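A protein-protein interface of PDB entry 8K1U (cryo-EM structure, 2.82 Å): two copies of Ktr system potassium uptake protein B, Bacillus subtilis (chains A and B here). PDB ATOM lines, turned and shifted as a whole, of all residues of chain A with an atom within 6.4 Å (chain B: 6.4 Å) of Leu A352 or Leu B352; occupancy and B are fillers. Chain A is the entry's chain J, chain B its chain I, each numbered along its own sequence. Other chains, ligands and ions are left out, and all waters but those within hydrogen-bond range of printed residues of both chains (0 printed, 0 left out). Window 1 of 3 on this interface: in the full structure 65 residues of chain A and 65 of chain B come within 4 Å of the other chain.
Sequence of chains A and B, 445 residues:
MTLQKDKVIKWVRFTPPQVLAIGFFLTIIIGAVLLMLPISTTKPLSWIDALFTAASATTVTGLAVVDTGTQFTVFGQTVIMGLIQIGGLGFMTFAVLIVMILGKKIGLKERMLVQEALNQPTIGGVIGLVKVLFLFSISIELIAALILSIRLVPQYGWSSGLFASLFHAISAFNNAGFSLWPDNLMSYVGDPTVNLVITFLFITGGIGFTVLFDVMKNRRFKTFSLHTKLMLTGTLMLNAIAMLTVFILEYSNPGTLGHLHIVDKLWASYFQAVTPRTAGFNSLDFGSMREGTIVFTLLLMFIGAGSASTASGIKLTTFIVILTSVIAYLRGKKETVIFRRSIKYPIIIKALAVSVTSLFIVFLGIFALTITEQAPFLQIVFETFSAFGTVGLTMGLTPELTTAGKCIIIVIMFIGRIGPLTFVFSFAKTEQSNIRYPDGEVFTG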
ATOM      1  N   THR A 318      13.860   8.824 -20.087  1.00  0.00           N
ATOM      2  CA  THR A 318      12.684   9.617 -19.738  1.00  0.00           C
ATOM      3  C   THR A 318      13.040  11.090 -19.581  1.00  0.00           C
ATOM      4  O   THR A 318      12.301  11.969 -20.040  1.00  0.00           O
ATOM      5  CB  THR A 318      12.051   9.074 -18.454  1.00  0.00           C
ATOM      6  OG1 THR A 318      11.705   7.696 -18.634  1.00  0.00           O
ATOM      7  CG2 THR A 318      10.797   9.859 -18.092  1.00  0.00           C
ATOM      8  N   ILE A 322      11.706  14.151 -22.278  1.00  0.00           N
ATOM      9  CA  ILE A 322      10.967  15.322 -21.812  1.00  0.00           C
ATOM     10  C   ILE A 322      11.749  16.599 -22.091  1.00  0.00           C
ATOM     11  O   ILE A 322      11.182  17.603 -22.540  1.00  0.00           O
ATOM     12  CB  ILE A 322      10.628  15.176 -20.318  1.00  0.00           C
ATOM     13  CG1 ILE A 322       9.698  13.982 -20.100  1.00  0.00           C
ATOM     14  CG2 ILE A 322       9.988  16.447 -19.778  1.00  0.00           C
ATOM     15  CD1 ILE A 322       9.316  13.773 -18.659  1.00  0.00           C
ATOM     16  N   SER A 325      11.639  17.453 -25.778  1.00  0.00           N
ATOM     17  CA  SER A 325      10.300  17.854 -26.198  1.00  0.00           C
ATOM     18  C   SER A 325      10.013  19.307 -25.836  1.00  0.00           C
ATOM     19  O   SER A 325       9.347  20.020 -26.595  1.00  0.00           O
ATOM     20  CB  SER A 325       9.257  16.929 -25.572  1.00  0.00           C
ATOM     21  OG  SER A 325       7.947  17.298 -25.967  1.00  0.00           O
ATOM     22  N   VAL A 326      10.498  19.759 -24.678  1.00  0.00           N
ATOM     23  CA  VAL A 326      10.308  21.152 -24.285  1.00  0.00           C
ATOM     24  C   VAL A 326      11.150  22.074 -25.158  1.00  0.00           C
ATOM     25  O   VAL A 326      10.673  23.118 -25.619  1.00  0.00           O
ATOM     26  CB  VAL A 326      10.629  21.333 -22.789  1.00  0.00           C
ATOM     27  CG1 VAL A 326      10.515  22.794 -22.388  1.00  0.00           C
ATOM     28  CG2 VAL A 326       9.699  20.478 -21.946  1.00  0.00           C
ATOM     29  N   ILE A 347       5.124   7.885 -26.800  1.00  0.00           N
ATOM     30  CA  ILE A 347       6.356   7.911 -26.018  1.00  0.00           C
ATOM     31  C   ILE A 347       6.396   9.148 -25.127  1.00  0.00           C
ATOM     32  O   ILE A 347       6.854   9.090 -23.980  1.00  0.00           O
ATOM     33  CB  ILE A 347       7.579   7.837 -26.950  1.00  0.00           C
ATOM     34  CG1 ILE A 347       7.465   6.630 -27.883  1.00  0.00           C
ATOM     35  CG2 ILE A 347       8.867   7.762 -26.146  1.00  0.00           C
ATOM     36  CD1 ILE A 347       7.418   5.302 -27.159  1.00  0.00           C
ATOM     37  N   ILE A 348       5.915  10.284 -25.640  1.00  0.00           N
ATOM     38  CA  ILE A 348       5.954  11.533 -24.883  1.00  0.00           C
ATOM     39  C   ILE A 348       5.023  11.462 -23.676  1.00  0.00           C
ATOM     40  O   ILE A 348       5.390  11.863 -22.565  1.00  0.00           O
ATOM     41  CB  ILE A 348       5.601  12.723 -25.794  1.00  0.00           C
ATOM     42  CG1 ILE A 348       6.511  12.752 -27.024  1.00  0.00           C
ATOM     43  CG2 ILE A 348       5.696  14.032 -25.026  1.00  0.00           C
ATOM     44  CD1 ILE A 348       7.956  13.061 -26.712  1.00  0.00           C
ATOM     45  N   ILE A 349       3.804  10.952 -23.876  1.00  0.00           N
ATOM     46  CA  ILE A 349       2.818  10.949 -22.798  1.00  0.00           C
ATOM     47  C   ILE A 349       3.195   9.948 -21.709  1.00  0.00           C
ATOM     48  O   ILE A 349       2.892  10.164 -20.529  1.00  0.00           O
ATOM     49  CB  ILE A 349       1.405  10.696 -23.365  1.00  0.00           C
ATOM     50  CG1 ILE A 349       0.338  10.879 -22.280  1.00  0.00           C
ATOM     51  CG2 ILE A 349       1.295   9.318 -23.999  1.00  0.00           C
ATOM     52  CD1 ILE A 349      -1.075  10.661 -22.770  1.00  0.00           C
ATOM     53  N   LYS A 350       3.864   8.848 -22.070  1.00  0.00           N
ATOM     54  CA  LYS A 350       4.307   7.898 -21.054  1.00  0.00           C
ATOM     55  C   LYS A 350       5.407   8.495 -20.185  1.00  0.00           C
ATOM     56  O   LYS A 350       5.402   8.318 -18.962  1.00  0.00           O
ATOM     57  CB  LYS A 350       4.785   6.602 -21.709  1.00  0.00           C
ATOM     58  CG  LYS A 350       5.200   5.532 -20.711  1.00  0.00           C
ATOM     59  CD  LYS A 350       5.637   4.256 -21.404  1.00  0.00           C
ATOM     60  CE  LYS A 350       6.024   3.189 -20.394  1.00  0.00           C
ATOM     61  NZ  LYS A 350       6.444   1.926 -21.059  1.00  0.00           N
ATOM     62  N   ALA A 351       6.354   9.210 -20.800  1.00  0.00           N
ATOM     63  CA  ALA A 351       7.374   9.913 -20.028  1.00  0.00           C
ATOM     64  C   ALA A 351       6.765  11.029 -19.190  1.00  0.00           C
ATOM     65  O   ALA A 351       7.237  11.295 -18.077  1.00  0.00           O
ATOM     66  CB  ALA A 351       8.448  10.470 -20.960  1.00  0.00           C
ATOM     67  N   LEU A 352       5.730  11.693 -19.709  1.00  0.00           N
ATOM     68  CA  LEU A 352       5.012  12.698 -18.932  1.00  0.00           C
ATOM     69  C   LEU A 352       4.337  12.071 -17.718  1.00  0.00           C
ATOM     70  O   LEU A 352       4.329  12.658 -16.629  1.00  0.00           O
ATOM     71  CB  LEU A 352       3.993  13.406 -19.829  1.00  0.00           C
ATOM     72  CG  LEU A 352       3.129  14.583 -19.350  1.00  0.00           C
ATOM     73  CD1 LEU A 352       1.782  14.114 -18.810  1.00  0.00           C
ATOM     74  CD2 LEU A 352       3.854  15.440 -18.324  1.00  0.00           C
ATOM     75  N   ALA A 353       3.768  10.875 -17.883  1.00  0.00           N
ATOM     76  CA  ALA A 353       3.109  10.207 -16.767  1.00  0.00           C
ATOM     77  C   ALA A 353       4.106   9.731 -15.719  1.00  0.00           C
ATOM     78  O   ALA A 353       3.790   9.732 -14.524  1.00  0.00           O
ATOM     79  CB  ALA A 353       2.275   9.033 -17.274  1.00  0.00           C
ATOM     80  N   VAL A 354       5.300   9.310 -16.140  1.00  0.00           N
ATOM     81  CA  VAL A 354       6.304   8.831 -15.192  1.00  0.00           C
ATOM     82  C   VAL A 354       6.805   9.973 -14.316  1.00  0.00           C
ATOM     83  O   VAL A 354       6.896   9.843 -13.091  1.00  0.00           O
ATOM     84  CB  VAL A 354       7.462   8.141 -15.938  1.00  0.00           C
ATOM     85  CG1 VAL A 354       8.634   7.899 -15.001  1.00  0.00           C
ATOM     86  CG2 VAL A 354       6.998   6.828 -16.542  1.00  0.00           C
ATOM     87  N   SER A 355       7.118  11.118 -14.930  1.00  0.00           N
ATOM     88  CA  SER A 355       7.752  12.207 -14.194  1.00  0.00           C
ATOM     89  C   SER A 355       6.782  12.889 -13.237  1.00  0.00           C
ATOM     90  O   SER A 355       7.163  13.258 -12.120  1.00  0.00           O
ATOM     91  CB  SER A 355       8.339  13.224 -15.170  1.00  0.00           C
ATOM     92  OG  SER A 355       8.983  14.279 -14.478  1.00  0.00           O
ATOM     93  N   VAL A 356       5.529  13.079 -13.658  1.00  0.00           N
ATOM     94  CA  VAL A 356       4.556  13.757 -12.805  1.00  0.00           C
ATOM     95  C   VAL A 356       4.176  12.879 -11.618  1.00  0.00           C
ATOM     96  O   VAL A 356       4.085  13.355 -10.481  1.00  0.00           O
ATOM     97  CB  VAL A 356       3.322  14.172 -13.628  1.00  0.00           C
ATOM     98  CG1 VAL A 356       2.220  14.696 -12.720  1.00  0.00           C
ATOM     99  CG2 VAL A 356       3.706  15.227 -14.647  1.00  0.00           C
ATOM    100  N   THR A 357       3.952  11.585 -11.862  1.00  0.00           N
ATOM    101  CA  THR A 357       3.615  10.674 -10.772  1.00  0.00           C
ATOM    102  C   THR A 357       4.783  10.510  -9.808  1.00  0.00           C
ATOM    103  O   THR A 357       4.577  10.389  -8.595  1.00  0.00           O
ATOM    104  CB  THR A 357       3.183   9.318 -11.331  1.00  0.00           C
ATOM    105  OG1 THR A 357       2.287   9.520 -12.432  1.00  0.00           O
ATOM    106  CG2 THR A 357       2.471   8.505 -10.263  1.00  0.00           C
ATOM    107  N   THR B 318      -3.295  25.373 -15.849  1.00  0.00           N
ATOM    108  CA  THR B 318      -2.141  24.571 -16.245  1.00  0.00           C
ATOM    109  C   THR B 318      -1.977  23.357 -15.338  1.00  0.00           C
ATOM    110  O   THR B 318      -1.690  22.251 -15.812  1.00  0.00           O
ATOM    111  CB  THR B 318      -0.875  25.432 -16.228  1.00  0.00           C
ATOM    112  OG1 THR B 318      -1.044  26.553 -17.104  1.00  0.00           O
ATOM    113  CG2 THR B 318       0.336  24.627 -16.677  1.00  0.00           C
ATOM    114  N   ILE B 322      -2.592  19.317 -16.654  1.00  0.00           N
ATOM    115  CA  ILE B 322      -1.557  18.295 -16.514  1.00  0.00           C
ATOM    116  C   ILE B 322      -2.027  17.173 -15.597  1.00  0.00           C
ATOM    117  O   ILE B 322      -1.819  15.989 -15.890  1.00  0.00           O
ATOM    118  CB  ILE B 322      -0.246  18.929 -16.013  1.00  0.00           C
ATOM    119  CG1 ILE B 322       0.287  19.926 -17.041  1.00  0.00           C
ATOM    120  CG2 ILE B 322       0.799  17.861 -15.723  1.00  0.00           C
ATOM    121  CD1 ILE B 322       1.572  20.590 -16.625  1.00  0.00           C
ATOM    122  N   SER B 325      -4.567  14.987 -17.361  1.00  0.00           N
ATOM    123  CA  SER B 325      -3.959  14.221 -18.443  1.00  0.00           C
ATOM    124  C   SER B 325      -3.238  12.985 -17.916  1.00  0.00           C
ATOM    125  O   SER B 325      -3.252  11.931 -18.560  1.00  0.00           O
ATOM    126  CB  SER B 325      -2.998  15.106 -19.235  1.00  0.00           C
ATOM    127  OG  SER B 325      -2.394  14.384 -20.294  1.00  0.00           O
ATOM    128  N   VAL B 326      -2.592  13.100 -16.754  1.00  0.00           N
ATOM    129  CA  VAL B 326      -1.920  11.949 -16.158  1.00  0.00           C
ATOM    130  C   VAL B 326      -2.941  10.935 -15.654  1.00  0.00           C
ATOM    131  O   VAL B 326      -2.792   9.727 -15.869  1.00  0.00           O
ATOM    132  CB  VAL B 326      -0.969  12.408 -15.039  1.00  0.00           C
ATOM    133  CG1 VAL B 326      -0.326  11.209 -14.356  1.00  0.00           C
ATOM    134  CG2 VAL B 326       0.097  13.331 -15.599  1.00  0.00           C
ATOM    135  N   ILE B 347      -2.962  22.103 -26.406  1.00  0.00           N
ATOM    136  CA  ILE B 347      -3.152  22.599 -25.047  1.00  0.00           C
ATOM    137  C   ILE B 347      -2.281  21.818 -24.068  1.00  0.00           C
ATOM    138  O   ILE B 347      -1.721  22.388 -23.123  1.00  0.00           O
ATOM    139  CB  ILE B 347      -4.641  22.536 -24.663  1.00  0.00           C
ATOM    140  CG1 ILE B 347      -5.491  23.261 -25.708  1.00  0.00           C
ATOM    141  CG2 ILE B 347      -4.869  23.143 -23.287  1.00  0.00           C
ATOM    142  CD1 ILE B 347      -5.162  24.731 -25.851  1.00  0.00           C
ATOM    143  N   ILE B 348      -2.152  20.506 -24.281  1.00  0.00           N
ATOM    144  CA  ILE B 348      -1.378  19.664 -23.371  1.00  0.00           C
ATOM    145  C   ILE B 348       0.105  20.014 -23.442  1.00  0.00           C
ATOM    146  O   ILE B 348       0.780  20.135 -22.413  1.00  0.00           O
ATOM    147  CB  ILE B 348      -1.618  18.177 -23.684  1.00  0.00           C
ATOM    148  CG1 ILE B 348      -3.114  17.852 -23.656  1.00  0.00           C
ATOM    149  CG2 ILE B 348      -0.860  17.293 -22.702  1.00  0.00           C
ATOM    150  CD1 ILE B 348      -3.740  17.952 -22.286  1.00  0.00           C
ATOM    151  N   ILE B 349       0.636  20.179 -24.657  1.00  0.00           N
ATOM    152  CA  ILE B 349       2.070  20.408 -24.814  1.00  0.00           C
ATOM    153  C   ILE B 349       2.463  21.797 -24.316  1.00  0.00           C
ATOM    154  O   ILE B 349       3.582  21.990 -23.823  1.00  0.00           O
ATOM    155  CB  ILE B 349       2.495  20.167 -26.279  1.00  0.00           C
ATOM    156  CG1 ILE B 349       4.019  20.215 -26.421  1.00  0.00           C
ATOM    157  CG2 ILE B 349       1.834  21.160 -27.223  1.00  0.00           C
ATOM    158  CD1 ILE B 349       4.509  19.971 -27.832  1.00  0.00           C
ATOM    159  N   LYS B 350       1.566  22.782 -24.423  1.00  0.00           N
ATOM    160  CA  LYS B 350       1.871  24.108 -23.896  1.00  0.00           C
ATOM    161  C   LYS B 350       1.936  24.094 -22.374  1.00  0.00           C
ATOM    162  O   LYS B 350       2.824  24.715 -21.781  1.00  0.00           O
ATOM    163  CB  LYS B 350       0.839  25.125 -24.380  1.00  0.00           C
ATOM    164  CG  LYS B 350       1.127  26.549 -23.930  1.00  0.00           C
ATOM    165  CD  LYS B 350       0.094  27.526 -24.458  1.00  0.00           C
ATOM    166  CE  LYS B 350       0.410  28.946 -24.021  1.00  0.00           C
ATOM    167  NZ  LYS B 350      -0.588  29.919 -24.540  1.00  0.00           N
ATOM    168  N   ALA B 351       1.006  23.386 -21.727  1.00  0.00           N
ATOM    169  CA  ALA B 351       1.067  23.225 -20.279  1.00  0.00           C
ATOM    170  C   ALA B 351       2.287  22.417 -19.861  1.00  0.00           C
ATOM    171  O   ALA B 351       2.872  22.681 -18.803  1.00  0.00           O
ATOM    172  CB  ALA B 351      -0.212  22.564 -19.768  1.00  0.00           C
ATOM    173  N   LEU B 352       2.677  21.429 -20.670  1.00  0.00           N
ATOM    174  CA  LEU B 352       3.901  20.678 -20.410  1.00  0.00           C
ATOM    175  C   LEU B 352       5.126  21.582 -20.494  1.00  0.00           C
ATOM    176  O   LEU B 352       6.056  21.457 -19.689  1.00  0.00           O
ATOM    177  CB  LEU B 352       4.004  19.511 -21.397  1.00  0.00           C
ATOM    178  CG  LEU B 352       5.129  18.465 -21.343  1.00  0.00           C
ATOM    179  CD1 LEU B 352       6.303  18.850 -22.238  1.00  0.00           C
ATOM    180  CD2 LEU B 352       5.597  18.207 -19.919  1.00  0.00           C
ATOM    181  N   ALA B 353       5.142  22.502 -21.461  1.00  0.00           N
ATOM    182  CA  ALA B 353       6.275  23.409 -21.600  1.00  0.00           C
ATOM    183  C   ALA B 353       6.342  24.419 -20.463  1.00  0.00           C
ATOM    184  O   ALA B 353       7.439  24.811 -20.052  1.00  0.00           O
ATOM    185  CB  ALA B 353       6.208  24.133 -22.944  1.00  0.00           C
ATOM    186  N   VAL B 354       5.189  24.860 -19.952  1.00  0.00           N
ATOM    187  CA  VAL B 354       5.176  25.836 -18.865  1.00  0.00           C
ATOM    188  C   VAL B 354       5.725  25.219 -17.584  1.00  0.00           C
ATOM    189  O   VAL B 354       6.563  25.817 -16.899  1.00  0.00           O
ATOM    190  CB  VAL B 354       3.754  26.392 -18.659  1.00  0.00           C
ATOM    191  CG1 VAL B 354       3.669  27.179 -17.362  1.00  0.00           C
ATOM    192  CG2 VAL B 354       3.353  27.271 -19.829  1.00  0.00           C
ATOM    193  N   SER B 355       5.278  24.006 -17.252  1.00  0.00           N
ATOM    194  CA  SER B 355       5.628  23.409 -15.965  1.00  0.00           C
ATOM    195  C   SER B 355       7.087  22.974 -15.919  1.00  0.00           C
ATOM    196  O   SER B 355       7.752  23.130 -14.888  1.00  0.00           O
ATOM    197  CB  SER B 355       4.710  22.225 -15.671  1.00  0.00           C
ATOM    198  OG  SER B 355       5.016  21.645 -14.416  1.00  0.00           O
ATOM    199  N   VAL B 356       7.601  22.415 -17.017  1.00  0.00           N
ATOM    200  CA  VAL B 356       8.984  21.943 -17.029  1.00  0.00           C
ATOM    201  C   VAL B 356       9.954  23.118 -17.001  1.00  0.00           C
ATOM    202  O   VAL B 356      10.953  23.099 -16.272  1.00  0.00           O
ATOM    203  CB  VAL B 356       9.225  21.032 -18.247  1.00  0.00           C
ATOM    204  CG1 VAL B 356      10.702  20.695 -18.384  1.00  0.00           C
ATOM    205  CG2 VAL B 356       8.412  19.759 -18.115  1.00  0.00           C
ATOM    206  N   THR B 357       9.675  24.161 -17.787  1.00  0.00           N
ATOM    207  CA  THR B 357      10.539  25.337 -17.792  1.00  0.00           C
ATOM    208  C   THR B 357      10.492  26.064 -16.454  1.00  0.00           C
ATOM    209  O   THR B 357      11.510  26.592 -15.994  1.00  0.00           O
ATOM    210  CB  THR B 357      10.144  26.279 -18.930  1.00  0.00           C
ATOM    211  OG1 THR B 357       9.924  25.518 -20.124  1.00  0.00           O
ATOM    212  CG2 THR B 357      11.248  27.291 -19.190  1.00  0.00           C
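Of the 15 printed residues of chain A, 4 touch a printed residue of chain B.
Printed residues of chain A that touch a printed residue of chain B: Val A326, Leu A352, Val A356 and Thr A357.
Of the 15 printed residues of chain B, 4 touch a printed residue of chain A.
Hydrophobic or aromatic side chains of chain B that line the printed part of chain A: Val B326, Leu B352 and Val B356.
Along chain B the printed residues that touch a printed residue of chain A span positions 326 to 357.
Among the printed residues, 7 pairs touch across the chains.
Among the printed residues, no Asp or Glu carboxylate lies within 4 Å of a Lys or Arg side-chain nitrogen of the other chain.
The backbone carbonyl oxygen (O) of Ala B353 is in hydrogen-bond range of the side-chain hydroxyl (OG1) of Thr B357, at 2.6 Å.
O of Ala A353 sits at hydrogen-bond distance from OG1 of Thr A357, at 2.6 Å.
Val A326 touches Leu B352, and with the chains exchanged Leu A352 touches Val B326.
Val A326 touches Val B356, and with the chains exchanged Val A356 touches Val B326.
Val A326 touches Thr B357, and with the chains exchanged Thr A357 touches Val B326.
Leu B352 touches its own counterpart, Leu A352.
Positions printed for both chains: 318, 322, 325, 326, 347, 348, 349, 350, 351, 352, 353, 354, 355, 356 and 357.
Of the 7 pairs that touch across the chains among the printed residues, 7 have their exchanged pair printed and touching as well.
Val A326 touches Leu B352 (CG2 to CD1, 3.8 Å).
Val A326 touches Val B356.
Val A326 touches Thr B357.
CD1 of Leu A352 touches CG2 of Val B326, 3.7 Å away.
Leu A352 touches Leu B352.
CG1 of Val A356 touches CG2 of Val B326, at 3.8 Å.
Thr A357 touches Val B326 (OG1 to CG1, 3.7 Å).
Of the printed residues of chain B, Val A326 touches Leu B352 (3.8 Å), Val B356 (3.7 Å) and Thr B357 (3.6 Å).
Of the printed residues of chain B, Leu A352 touches Val B326 and Leu B352.
Ser A355 touches none of the printed residues of chain B.
Of the printed residues of chain B, Thr A357 touches Val B326.
Ala B351 touches none of the printed residues of chain A.
The nearest residue of chain A that does not touch Leu B352 is Ser A325 (4.4 Å).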
